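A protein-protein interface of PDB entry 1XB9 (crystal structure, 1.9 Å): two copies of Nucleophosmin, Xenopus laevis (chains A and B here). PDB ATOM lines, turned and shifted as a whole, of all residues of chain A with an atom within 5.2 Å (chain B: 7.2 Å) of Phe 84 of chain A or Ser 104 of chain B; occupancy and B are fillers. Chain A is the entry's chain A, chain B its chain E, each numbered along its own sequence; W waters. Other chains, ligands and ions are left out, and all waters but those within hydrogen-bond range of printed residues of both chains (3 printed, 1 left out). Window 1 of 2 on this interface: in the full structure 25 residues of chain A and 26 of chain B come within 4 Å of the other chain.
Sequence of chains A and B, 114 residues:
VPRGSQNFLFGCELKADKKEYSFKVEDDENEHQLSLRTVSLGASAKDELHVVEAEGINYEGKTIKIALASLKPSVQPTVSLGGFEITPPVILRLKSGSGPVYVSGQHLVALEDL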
ATOM      1  N   LEU A  34       9.843  -6.897 -12.397  1.00  0.00           N
ATOM      2  CA  LEU A  34       9.980  -5.467 -12.200  1.00  0.00           C
ATOM      3  C   LEU A  34       8.566  -4.944 -11.951  1.00  0.00           C
ATOM      4  O   LEU A  34       7.611  -5.325 -12.655  1.00  0.00           O
ATOM      5  CB  LEU A  34      10.540  -4.944 -13.485  1.00  0.00           C
ATOM      6  CG  LEU A  34      11.667  -4.023 -13.560  1.00  0.00           C
ATOM      7  CD1 LEU A  34      12.788  -4.650 -12.677  1.00  0.00           C
ATOM      8  CD2 LEU A  34      12.038  -3.788 -15.010  1.00  0.00           C
ATOM      9  N   SER A  35       8.373  -4.061 -10.984  1.00  0.00           N
ATOM     10  CA  SER A  35       7.103  -3.365 -10.816  1.00  0.00           C
ATOM     11  C   SER A  35       7.410  -1.852 -11.021  1.00  0.00           C
ATOM     12  O   SER A  35       7.822  -1.215 -10.073  1.00  0.00           O
ATOM     13  CB  SER A  35       6.489  -3.633  -9.449  1.00  0.00           C
ATOM     14  OG  SER A  35       5.241  -3.005  -9.340  1.00  0.00           O
ATOM     15  N   LEU A  36       7.093  -1.306 -12.181  1.00  0.00           N
ATOM     16  CA  LEU A  36       7.310   0.126 -12.449  1.00  0.00           C
ATOM     17  C   LEU A  36       6.373   1.005 -11.633  1.00  0.00           C
ATOM     18  O   LEU A  36       5.139   0.838 -11.626  1.00  0.00           O
ATOM     19  CB  LEU A  36       7.230   0.460 -13.964  1.00  0.00           C
ATOM     20  CG  LEU A  36       8.143  -0.478 -14.793  1.00  0.00           C
ATOM     21  CD1 LEU A  36       8.258   0.005 -16.212  1.00  0.00           C
ATOM     22  CD2 LEU A  36       9.472  -0.530 -14.229  1.00  0.00           C
ATOM     23  N   ILE A  66       5.623  -0.875 -26.536  1.00  0.00           N
ATOM     24  CA  ILE A  66       4.435  -0.294 -25.897  1.00  0.00           C
ATOM     25  C   ILE A  66       4.927   1.031 -25.217  1.00  0.00           C
ATOM     26  O   ILE A  66       6.024   1.076 -24.621  1.00  0.00           O
ATOM     27  CB  ILE A  66       3.807  -1.267 -24.906  1.00  0.00           C
ATOM     28  CG1 ILE A  66       4.582  -1.406 -23.630  1.00  0.00           C
ATOM     29  CG2 ILE A  66       3.764  -2.725 -25.397  1.00  0.00           C
ATOM     30  CD1 ILE A  66       3.871  -2.154 -22.522  1.00  0.00           C
ATOM     31  N   ALA A  67       4.042   2.026 -25.241  1.00  0.00           N
ATOM     32  CA  ALA A  67       4.332   3.368 -24.869  1.00  0.00           C
ATOM     33  C   ALA A  67       3.939   3.308 -23.417  1.00  0.00           C
ATOM     34  O   ALA A  67       2.852   3.033 -23.126  1.00  0.00           O
ATOM     35  CB  ALA A  67       3.430   4.386 -25.631  1.00  0.00           C
ATOM     36  N   LEU A  68       4.839   3.585 -22.501  1.00  0.00           N
ATOM     37  CA  LEU A  68       4.491   3.661 -21.125  1.00  0.00           C
ATOM     38  C   LEU A  68       3.932   4.992 -20.690  1.00  0.00           C
ATOM     39  O   LEU A  68       3.036   4.976 -19.842  1.00  0.00           O
ATOM     40  CB  LEU A  68       5.653   3.303 -20.168  1.00  0.00           C
ATOM     41  CG  LEU A  68       6.272   1.872 -20.365  1.00  0.00           C
ATOM     42  CD1 LEU A  68       7.432   1.680 -19.432  1.00  0.00           C
ATOM     43  CD2 LEU A  68       5.215   0.664 -20.280  1.00  0.00           C
ATOM     44  N   LEU A  81       2.877   4.999 -12.439  1.00  0.00           N
ATOM     45  CA  LEU A  81       2.358   3.851 -13.138  1.00  0.00           C
ATOM     46  C   LEU A  81       1.616   2.870 -12.215  1.00  0.00           C
ATOM     47  O   LEU A  81       0.976   1.913 -12.705  1.00  0.00           O
ATOM     48  CB  LEU A  81       3.499   3.112 -13.924  1.00  0.00           C
ATOM     49  CG  LEU A  81       4.207   3.950 -14.906  1.00  0.00           C
ATOM     50  CD1 LEU A  81       5.393   3.264 -15.435  1.00  0.00           C
ATOM     51  CD2 LEU A  81       3.272   4.456 -16.068  1.00  0.00           C
ATOM     52  N   GLY A  82       1.769   3.017 -10.873  1.00  0.00           N
ATOM     53  CA  GLY A  82       1.013   2.210  -9.936  1.00  0.00           C
ATOM     54  C   GLY A  82       1.345   0.725  -9.860  1.00  0.00           C
ATOM     55  O   GLY A  82       0.569  -0.074  -9.300  1.00  0.00           O
ATOM     56  N   GLY A  83       2.539   0.330 -10.298  1.00  0.00           N
ATOM     57  CA  GLY A  83       2.912  -1.056 -10.234  1.00  0.00           C
ATOM     58  C   GLY A  83       2.637  -1.832 -11.484  1.00  0.00           C
ATOM     59  O   GLY A  83       1.904  -2.842 -11.487  1.00  0.00           O
ATOM     60  N   PHE A  84       3.229  -1.323 -12.571  1.00  0.00           N
ATOM     61  CA  PHE A  84       3.126  -1.971 -13.873  1.00  0.00           C
ATOM     62  C   PHE A  84       4.104  -3.101 -13.819  1.00  0.00           C
ATOM     63  O   PHE A  84       5.309  -2.918 -13.921  1.00  0.00           O
ATOM     64  CB  PHE A  84       3.411  -0.929 -14.907  1.00  0.00           C
ATOM     65  CG  PHE A  84       3.154  -1.325 -16.314  1.00  0.00           C
ATOM     66  CD1 PHE A  84       2.850  -0.352 -17.226  1.00  0.00           C
ATOM     67  CD2 PHE A  84       3.267  -2.608 -16.742  1.00  0.00           C
ATOM     68  CE1 PHE A  84       2.556  -0.677 -18.517  1.00  0.00           C
ATOM     69  CE2 PHE A  84       3.038  -2.932 -18.083  1.00  0.00           C
ATOM     70  CZ  PHE A  84       2.689  -1.980 -18.962  1.00  0.00           C
ATOM     71  N   GLU A  85       3.574  -4.302 -13.613  1.00  0.00           N
ATOM     72  CA  GLU A  85       4.422  -5.477 -13.491  1.00  0.00           C
ATOM     73  C   GLU A  85       4.918  -5.996 -14.825  1.00  0.00           C
ATOM     74  O   GLU A  85       4.144  -6.187 -15.788  1.00  0.00           O
ATOM     75  CB  GLU A  85       3.731  -6.538 -12.679  1.00  0.00           C
ATOM     76  CG  GLU A  85       3.554  -6.072 -11.227  1.00  0.00           C
ATOM     77  CD  GLU A  85       3.317  -7.179 -10.225  1.00  0.00           C
ATOM     78  OE1 GLU A  85       4.313  -7.688  -9.640  1.00  0.00           O
ATOM     79  OE2 GLU A  85       2.167  -7.489  -9.964  1.00  0.00           O
ATOM     80  N   ILE A  86       6.230  -6.175 -14.953  1.00  0.00           N
ATOM     81  CA  ILE A  86       6.785  -6.701 -16.233  1.00  0.00           C
ATOM     82  C   ILE A  86       7.758  -7.862 -15.951  1.00  0.00           C
ATOM     83  O   ILE A  86       8.604  -7.812 -15.018  1.00  0.00           O
ATOM     84  CB  ILE A  86       7.625  -5.576 -16.940  1.00  0.00           C
ATOM     85  CG1 ILE A  86       6.695  -4.489 -17.428  1.00  0.00           C
ATOM     86  CG2 ILE A  86       8.469  -6.108 -18.090  1.00  0.00           C
ATOM     87  CD1 ILE A  86       7.331  -3.259 -17.864  1.00  0.00           C
ATOM     88  N   ASN B   7       2.588 -13.442 -17.184  1.00  0.00           N
ATOM     89  CA  ASN B   7       2.356 -11.964 -17.360  1.00  0.00           C
ATOM     90  C   ASN B   7       3.065 -11.493 -18.590  1.00  0.00           C
ATOM     91  O   ASN B   7       4.271 -11.597 -18.657  1.00  0.00           O
ATOM     92  CB  ASN B   7       2.950 -11.273 -16.154  1.00  0.00           C
ATOM     93  CG  ASN B   7       2.784  -9.790 -16.172  1.00  0.00           C
ATOM     94  OD1 ASN B   7       1.910  -9.287 -16.885  1.00  0.00           O
ATOM     95  ND2 ASN B   7       3.729  -9.054 -15.511  1.00  0.00           N
ATOM     96  N   PHE B   8       2.384 -11.008 -19.598  1.00  0.00           N
ATOM     97  CA  PHE B   8       3.044 -10.532 -20.793  1.00  0.00           C
ATOM     98  C   PHE B   8       2.726  -9.071 -21.007  1.00  0.00           C
ATOM     99  O   PHE B   8       1.674  -8.636 -20.608  1.00  0.00           O
ATOM    100  CB  PHE B   8       2.510 -11.310 -22.036  1.00  0.00           C
ATOM    101  CG  PHE B   8       2.702 -12.835 -21.931  1.00  0.00           C
ATOM    102  CD1 PHE B   8       1.687 -13.664 -21.425  1.00  0.00           C
ATOM    103  CD2 PHE B   8       3.905 -13.391 -22.206  1.00  0.00           C
ATOM    104  CE1 PHE B   8       1.817 -15.052 -21.383  1.00  0.00           C
ATOM    105  CE2 PHE B   8       4.037 -14.753 -22.137  1.00  0.00           C
ATOM    106  CZ  PHE B   8       2.979 -15.563 -21.685  1.00  0.00           C
ATOM    107  N   LEU B   9       3.598  -8.366 -21.720  1.00  0.00           N
ATOM    108  CA  LEU B   9       3.345  -7.040 -22.207  1.00  0.00           C
ATOM    109  C   LEU B   9       2.128  -6.993 -23.119  1.00  0.00           C
ATOM    110  O   LEU B   9       1.884  -7.904 -23.940  1.00  0.00           O
ATOM    111  CB  LEU B   9       4.548  -6.472 -22.949  1.00  0.00           C
ATOM    112  CG  LEU B   9       5.702  -5.956 -22.133  1.00  0.00           C
ATOM    113  CD1 LEU B   9       6.569  -5.271 -23.123  1.00  0.00           C
ATOM    114  CD2 LEU B   9       5.155  -4.965 -21.037  1.00  0.00           C
ATOM    115  N   PHE B  10       1.374  -5.929 -22.963  1.00  0.00           N
ATOM    116  CA  PHE B  10       0.257  -5.567 -23.872  1.00  0.00           C
ATOM    117  C   PHE B  10       0.288  -4.105 -24.345  1.00  0.00           C
ATOM    118  O   PHE B  10       0.508  -3.249 -23.554  1.00  0.00           O
ATOM    119  CB  PHE B  10      -1.105  -5.857 -23.244  1.00  0.00           C
ATOM    120  CG  PHE B  10      -2.244  -5.351 -24.089  1.00  0.00           C
ATOM    121  CD1 PHE B  10      -2.590  -6.031 -25.252  1.00  0.00           C
ATOM    122  CD2 PHE B  10      -2.762  -4.093 -23.869  1.00  0.00           C
ATOM    123  CE1 PHE B  10      -3.558  -5.529 -26.116  1.00  0.00           C
ATOM    124  CE2 PHE B  10      -3.746  -3.560 -24.679  1.00  0.00           C
ATOM    125  CZ  PHE B  10      -4.151  -4.266 -25.838  1.00  0.00           C
ATOM    126  N   GLY B  11       0.054  -3.844 -25.643  1.00  0.00           N
ATOM    127  CA  GLY B  11      -0.108  -2.467 -26.000  1.00  0.00           C
ATOM    128  C   GLY B  11      -0.769  -2.320 -27.369  1.00  0.00           C
ATOM    129  O   GLY B  11      -0.700  -3.311 -28.176  1.00  0.00           O
ATOM    130  N   CYS B  12      -1.263  -1.126 -27.630  1.00  0.00           N
ATOM    131  CA  CYS B  12      -1.713  -0.815 -28.958  1.00  0.00           C
ATOM    132  C   CYS B  12      -1.615   0.626 -29.230  1.00  0.00           C
ATOM    133  O   CYS B  12      -1.567   1.423 -28.320  1.00  0.00           O
ATOM    134  CB  CYS B  12      -3.151  -1.274 -29.180  1.00  0.00           C
ATOM    135  SG  CYS B  12      -4.431  -0.582 -28.239  1.00  0.00           S
ATOM    136  N   LEU B  34      -6.931  -8.727 -19.539  1.00  0.00           N
ATOM    137  CA  LEU B  34      -6.158  -7.595 -20.071  1.00  0.00           C
ATOM    138  C   LEU B  34      -6.236  -6.545 -18.964  1.00  0.00           C
ATOM    139  O   LEU B  34      -7.368  -6.246 -18.594  1.00  0.00           O
ATOM    140  CB  LEU B  34      -6.789  -7.248 -21.433  1.00  0.00           C
ATOM    141  CG  LEU B  34      -6.327  -6.006 -22.089  1.00  0.00           C
ATOM    142  CD1 LEU B  34      -4.915  -6.315 -22.587  1.00  0.00           C
ATOM    143  CD2 LEU B  34      -7.159  -5.481 -23.162  1.00  0.00           C
ATOM    144  N   SER B  35      -5.093  -6.249 -18.289  1.00  0.00           N
ATOM    145  CA  SER B  35      -4.989  -5.281 -17.231  1.00  0.00           C
ATOM    146  C   SER B  35      -4.342  -4.000 -17.729  1.00  0.00           C
ATOM    147  O   SER B  35      -3.120  -3.961 -18.039  1.00  0.00           O
ATOM    148  CB  SER B  35      -4.166  -5.848 -16.148  1.00  0.00           C
ATOM    149  OG  SER B  35      -4.081  -4.914 -15.074  1.00  0.00           O
ATOM    150  N   LEU B  36      -5.176  -3.025 -17.993  1.00  0.00           N
ATOM    151  CA  LEU B  36      -4.773  -1.755 -18.606  1.00  0.00           C
ATOM    152  C   LEU B  36      -4.078  -0.841 -17.618  1.00  0.00           C
ATOM    153  O   LEU B  36      -4.537  -0.641 -16.521  1.00  0.00           O
ATOM    154  CB  LEU B  36      -5.910  -1.068 -19.268  1.00  0.00           C
ATOM    155  CG  LEU B  36      -6.569  -1.862 -20.362  1.00  0.00           C
ATOM    156  CD1 LEU B  36      -7.631  -1.065 -20.932  1.00  0.00           C
ATOM    157  CD2 LEU B  36      -5.600  -2.457 -21.354  1.00  0.00           C
ATOM    158  N   ARG B  37      -2.880  -0.385 -17.977  1.00  0.00           N
ATOM    159  CA  ARG B  37      -2.092   0.483 -17.108  1.00  0.00           C
ATOM    160  C   ARG B  37      -2.060   1.938 -17.527  1.00  0.00           C
ATOM    161  O   ARG B  37      -2.299   2.790 -16.657  1.00  0.00           O
ATOM    162  CB  ARG B  37      -0.690  -0.026 -16.995  1.00  0.00           C
ATOM    163  CG  ARG B  37      -0.677  -1.306 -16.163  1.00  0.00           C
ATOM    164  CD  ARG B  37      -0.538  -0.842 -14.705  1.00  0.00           C
ATOM    165  NE  ARG B  37      -0.860  -1.909 -13.966  1.00  0.00           N
ATOM    166  CZ  ARG B  37      -1.111  -1.852 -12.730  1.00  0.00           C
ATOM    167  NH1 ARG B  37      -0.901  -0.706 -12.026  1.00  0.00           N
ATOM    168  NH2 ARG B  37      -1.413  -2.990 -12.251  1.00  0.00           N
ATOM    169  N   THR B  38      -1.723   2.293 -18.774  1.00  0.00           N
ATOM    170  CA  THR B  38      -1.698   3.695 -19.111  1.00  0.00           C
ATOM    171  C   THR B  38      -2.299   3.997 -20.447  1.00  0.00           C
ATOM    172  O   THR B  38      -2.267   3.170 -21.322  1.00  0.00           O
ATOM    173  CB  THR B  38      -0.297   4.374 -19.062  1.00  0.00           C
ATOM    174  OG1 THR B  38       0.529   3.739 -20.026  1.00  0.00           O
ATOM    175  CG2 THR B  38       0.398   4.228 -17.695  1.00  0.00           C
ATOM    176  N   VAL B  39      -2.818   5.188 -20.612  1.00  0.00           N
ATOM    177  CA  VAL B  39      -3.177   5.755 -21.884  1.00  0.00           C
ATOM    178  C   VAL B  39      -2.318   7.003 -22.103  1.00  0.00           C
ATOM    179  O   VAL B  39      -2.243   7.828 -21.207  1.00  0.00           O
ATOM    180  CB  VAL B  39      -4.665   6.109 -21.913  1.00  0.00           C
ATOM    181  CG1 VAL B  39      -5.023   6.473 -23.281  1.00  0.00           C
ATOM    182  CG2 VAL B  39      -5.456   4.920 -21.388  1.00  0.00           C
ATOM    183  N   SER B  40      -1.684   7.178 -23.263  1.00  0.00           N
ATOM    184  CA  SER B  40      -0.738   8.285 -23.418  1.00  0.00           C
ATOM    185  C   SER B  40      -0.735   8.777 -24.860  1.00  0.00           C
ATOM    186  O   SER B  40      -0.967   7.979 -25.779  1.00  0.00           O
ATOM    187  CB  SER B  40       0.700   7.872 -23.082  1.00  0.00           C
ATOM    188  OG  SER B  40       1.059   6.860 -23.934  1.00  0.00           O
ATOM    189  N   VAL B  79      -2.579   9.341 -18.739  1.00  0.00           N
ATOM    190  CA  VAL B  79      -3.543   8.860 -17.823  1.00  0.00           C
ATOM    191  C   VAL B  79      -3.155   7.432 -17.382  1.00  0.00           C
ATOM    192  O   VAL B  79      -3.017   6.496 -18.204  1.00  0.00           O
ATOM    193  CB  VAL B  79      -4.965   8.922 -18.437  1.00  0.00           C
ATOM    194  CG1 VAL B  79      -5.886   8.270 -17.627  1.00  0.00           C
ATOM    195  CG2 VAL B  79      -5.510  10.354 -18.713  1.00  0.00           C
ATOM    196  N   LEU B  81      -4.288   4.157 -15.468  1.00  0.00           N
ATOM    197  CA  LEU B  81      -5.462   3.428 -15.055  1.00  0.00           C
ATOM    198  C   LEU B  81      -5.393   2.589 -13.818  1.00  0.00           C
ATOM    199  O   LEU B  81      -6.403   2.255 -13.248  1.00  0.00           O
ATOM    200  CB  LEU B  81      -5.856   2.532 -16.195  1.00  0.00           C
ATOM    201  CG  LEU B  81      -6.251   3.351 -17.407  1.00  0.00           C
ATOM    202  CD1 LEU B  81      -6.428   2.503 -18.632  1.00  0.00           C
ATOM    203  CD2 LEU B  81      -7.490   4.288 -17.202  1.00  0.00           C
ATOM    204  N   LEU B  92     -10.729  -1.587 -28.297  1.00  0.00           N
ATOM    205  CA  LEU B  92     -10.363  -0.243 -27.925  1.00  0.00           C
ATOM    206  C   LEU B  92     -10.390   0.665 -29.116  1.00  0.00           C
ATOM    207  O   LEU B  92      -9.858   0.329 -30.126  1.00  0.00           O
ATOM    208  CB  LEU B  92      -8.980  -0.147 -27.258  1.00  0.00           C
ATOM    209  CG  LEU B  92      -8.780  -1.137 -26.099  1.00  0.00           C
ATOM    210  CD1 LEU B  92      -7.273  -1.311 -25.751  1.00  0.00           C
ATOM    211  CD2 LEU B  92      -9.546  -0.848 -25.020  1.00  0.00           C
ATOM    212  N   TYR B 102      -1.688   5.799 -27.254  1.00  0.00           N
ATOM    213  CA  TYR B 102      -1.160   4.434 -26.945  1.00  0.00           C
ATOM    214  C   TYR B 102      -1.856   3.939 -25.733  1.00  0.00           C
ATOM    215  O   TYR B 102      -2.214   4.702 -24.842  1.00  0.00           O
ATOM    216  CB  TYR B 102       0.333   4.452 -26.732  1.00  0.00           C
ATOM    217  CG  TYR B 102       1.055   4.857 -27.996  1.00  0.00           C
ATOM    218  CD1 TYR B 102       1.217   6.239 -28.316  1.00  0.00           C
ATOM    219  CD2 TYR B 102       1.515   3.940 -28.881  1.00  0.00           C
ATOM    220  CE1 TYR B 102       1.862   6.668 -29.535  1.00  0.00           C
ATOM    221  CE2 TYR B 102       2.181   4.362 -30.133  1.00  0.00           C
ATOM    222  CZ  TYR B 102       2.303   5.670 -30.444  1.00  0.00           C
ATOM    223  OH  TYR B 102       2.876   6.011 -31.604  1.00  0.00           O
ATOM    224  N   VAL B 103      -2.106   2.628 -25.705  1.00  0.00           N
ATOM    225  CA  VAL B 103      -2.708   2.020 -24.529  1.00  0.00           C
ATOM    226  C   VAL B 103      -1.685   0.942 -24.175  1.00  0.00           C
ATOM    227  O   VAL B 103      -1.192   0.194 -25.051  1.00  0.00           O
ATOM    228  CB  VAL B 103      -4.124   1.428 -24.895  1.00  0.00           C
ATOM    229  CG1 VAL B 103      -4.612   0.696 -23.781  1.00  0.00           C
ATOM    230  CG2 VAL B 103      -5.081   2.465 -25.183  1.00  0.00           C
ATOM    231  N   SER B 104      -1.320   0.846 -22.909  1.00  0.00           N
ATOM    232  CA  SER B 104      -0.326  -0.121 -22.465  1.00  0.00           C
ATOM    233  C   SER B 104      -0.911  -0.886 -21.268  1.00  0.00           C
ATOM    234  O   SER B 104      -1.807  -0.395 -20.595  1.00  0.00           O
ATOM    235  CB  SER B 104       1.014   0.580 -22.103  1.00  0.00           C
ATOM    236  OG  SER B 104       0.867   1.211 -20.767  1.00  0.00           O
ATOM    237  N   GLY B 105      -0.479  -2.150 -21.098  1.00  0.00           N
ATOM    238  CA  GLY B 105      -0.805  -2.898 -19.908  1.00  0.00           C
ATOM    239  C   GLY B 105      -0.176  -4.258 -19.932  1.00  0.00           C
ATOM    240  O   GLY B 105       0.891  -4.509 -20.499  1.00  0.00           O
ATOM    241  N   GLN B 106      -0.893  -5.133 -19.284  1.00  0.00           N
ATOM    242  CA  GLN B 106      -0.466  -6.523 -19.089  1.00  0.00           C
ATOM    243  C   GLN B 106      -1.517  -7.459 -19.666  1.00  0.00           C
ATOM    244  O   GLN B 106      -2.681  -7.158 -19.667  1.00  0.00           O
ATOM    245  CB  GLN B 106      -0.181  -6.818 -17.647  1.00  0.00           C
ATOM    246  CG  GLN B 106       0.742  -5.845 -16.928  1.00  0.00           C
ATOM    247  CD  GLN B 106       0.745  -6.026 -15.370  1.00  0.00           C
ATOM    248  OE1 GLN B 106       0.821  -7.160 -14.868  1.00  0.00           O
ATOM    249  NE2 GLN B 106       0.753  -4.951 -14.637  1.00  0.00           N
HETATM  250  O   HOH W   1       0.327   4.392 -22.970  1.00  0.00           O
HETATM  251  O   HOH W   2       1.562   0.994 -26.498  1.00  0.00           O
HETATM  252  O   HOH W   3      -1.470  -2.086  -9.175  1.00  0.00           O
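N of Gly 105 of chain B sits at hydrogen-bond distance from O of Phe 10 of chain B (2.9 Å).
OD1 of Asn 7 of chain B sits close to OE1 of Gln 106 of chain B (3.1 Å).
The side-chain hydroxyl (OG1) of Thr 38 of chain B is in hydrogen-bond range of the side-chain hydroxyl (OG) of Ser 104 of chain B, at 2.7 Å.
O of Arg 37 of chain B sits at hydrogen-bond distance from N of Leu 81 of chain B, 2.7 Å away.
The backbone carbonyl oxygen of Ser 40 of chain B sits at hydrogen-bond distance from the backbone NH of Tyr 102 of chain B (2.7 Å).
N of Arg 37 of chain B lies within hydrogen-bond range of O of Ser 104 of chain B (2.8 Å).
Of the printed residues of chain B, Gly 82 of chain A touches Arg 37.
Gly 83 of chain A touches just these residues of chain B: Arg 37 (3.4 Å) and Gln 106 (3.96 Å).
Of chain B, only Arg 37, Ser 104, Gly 105 and Gln 106 come within 4 Å of Phe 84 of chain A.
Of the printed residues of chain B, Ile 86 of chain A touches Asn 7 (3.9 Å) and Leu 9 (3.95 Å).
Printed residues of chain A within 4 Å of Asn 7 of chain B: Glu 85 (2.9 Å) and Ile 86 (3.9 Å).
Leu 34 of chain B touches none of the printed residues of chain A.
Val 103 of chain B touches none of the printed residues of chain A.
Ser 104 of chain B touches just these residues of chain A: Ile 66, Ala 67 and Phe 84.
Of the printed residues of chain A, Gln 106 of chain B touches Gly 83 (3.96 Å), Phe 84 (3.9 Å) and Glu 85 (3.1 Å).
The nearest residue of chain B that does not touch Phe 84 of chain A is Leu 9 of chain B (4.2 Å).
CD1 of Ile 66 of chain A touches CD2 of Leu 9 of chain B, at 3.4 Å.
CD1 of Ile 66 of chain A touches O of Phe 10 of chain B (3.7 Å).
CB of Ser 104 of chain B touches CD1 of Ile 66 of chain A, 3.98 Å away.
CB of Ala 67 of chain A touches OG of Ser 40 of chain B (3.8 Å).
CD2 of Leu 81 of chain A touches CG2 of Thr 38 of chain B (3.3 Å).
Gln 106 of chain B touches Gly 83 of chain A.
Arg 37 of chain B touches Phe 84 of chain A.
Phe 84 of chain A touches Gly 105 of chain B (CZ to O, 3.5 Å).
Phe 84 of chain A touches Gln 106 of chain B.
ND2 of Asn 7 of chain B touches N of Ile 86 of chain A, at 3.9 Å.
The backbone carbonyl oxygen (O) of Leu 68 of chain A sits at hydrogen-bond distance from the side-chain hydroxyl (OG1) of Thr 38 of chain B (2.8 Å).
The guanidinium group (NH2) of Arg 37 of chain B lies within hydrogen-bond range of the backbone carbonyl oxygen (O) of Gly 83 of chain A (3.4 Å).
The backbone carbonyl oxygen (O) of Glu 85 of chain A is in hydrogen-bond range of the side-chain amide nitrogen (ND2) of Asn 7 of chain B, at 2.9 Å.
The side-chain amide nitrogen (NE2) of Gln 106 of chain B sits close to the backbone NH (N) of Glu 85 of chain A (3.1 Å).
The guanidinium group (NH1) of Arg 37 of chain B lies within hydrogen-bond range of the backbone carbonyl oxygen (O) of Gly 82 of chain A (3.2 Å).
The backbone carbonyl oxygen (O) of Leu 81 of chain A lies within hydrogen-bond range of the guanidinium group (NH1) of Arg 37 of chain B.
Hydrophobic or aromatic side chains of chain B within 4 Å of the printed part of chain A: Leu 9 and Tyr 102.
Printed residues of chain A that touch a printed residue of chain B: Ile 66, Ala 67, Leu 68, Leu 81, Gly 82, Gly 83, Phe 84, Glu 85 and Ile 86.
Along chain A the printed residues that touch a printed residue of chain B span positions 66 to 86.
Among the printed residues, no Asp or Glu carboxylate lies within 4 Å of a Lys or Arg side-chain nitrogen of the other chain.
Water W1 lies within hydrogen-bond range of the side-chain hydroxyl (OG) of Ser 40 of chain B, the backbone carbonyl oxygen (O) of Ala 67 of chain A, the side-chain hydroxyl (OG1) of Thr 38 of chain B and the backbone carbonyl oxygen (O) of Tyr 102 of chain B.
Water W3 lies within hydrogen-bond range of the backbone carbonyl oxygen of Gly 82 of chain A (2.9 Å) and the guanidinium group of Arg 37 of chain B (3.2 Å).
Water W2 lies within hydrogen-bond range of the backbone NH (N) of Ala 67 of chain A and the backbone carbonyl oxygen (O) of Val 103 of chain B.
Positions printed for both chains: 34, 35, 36 and 81.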
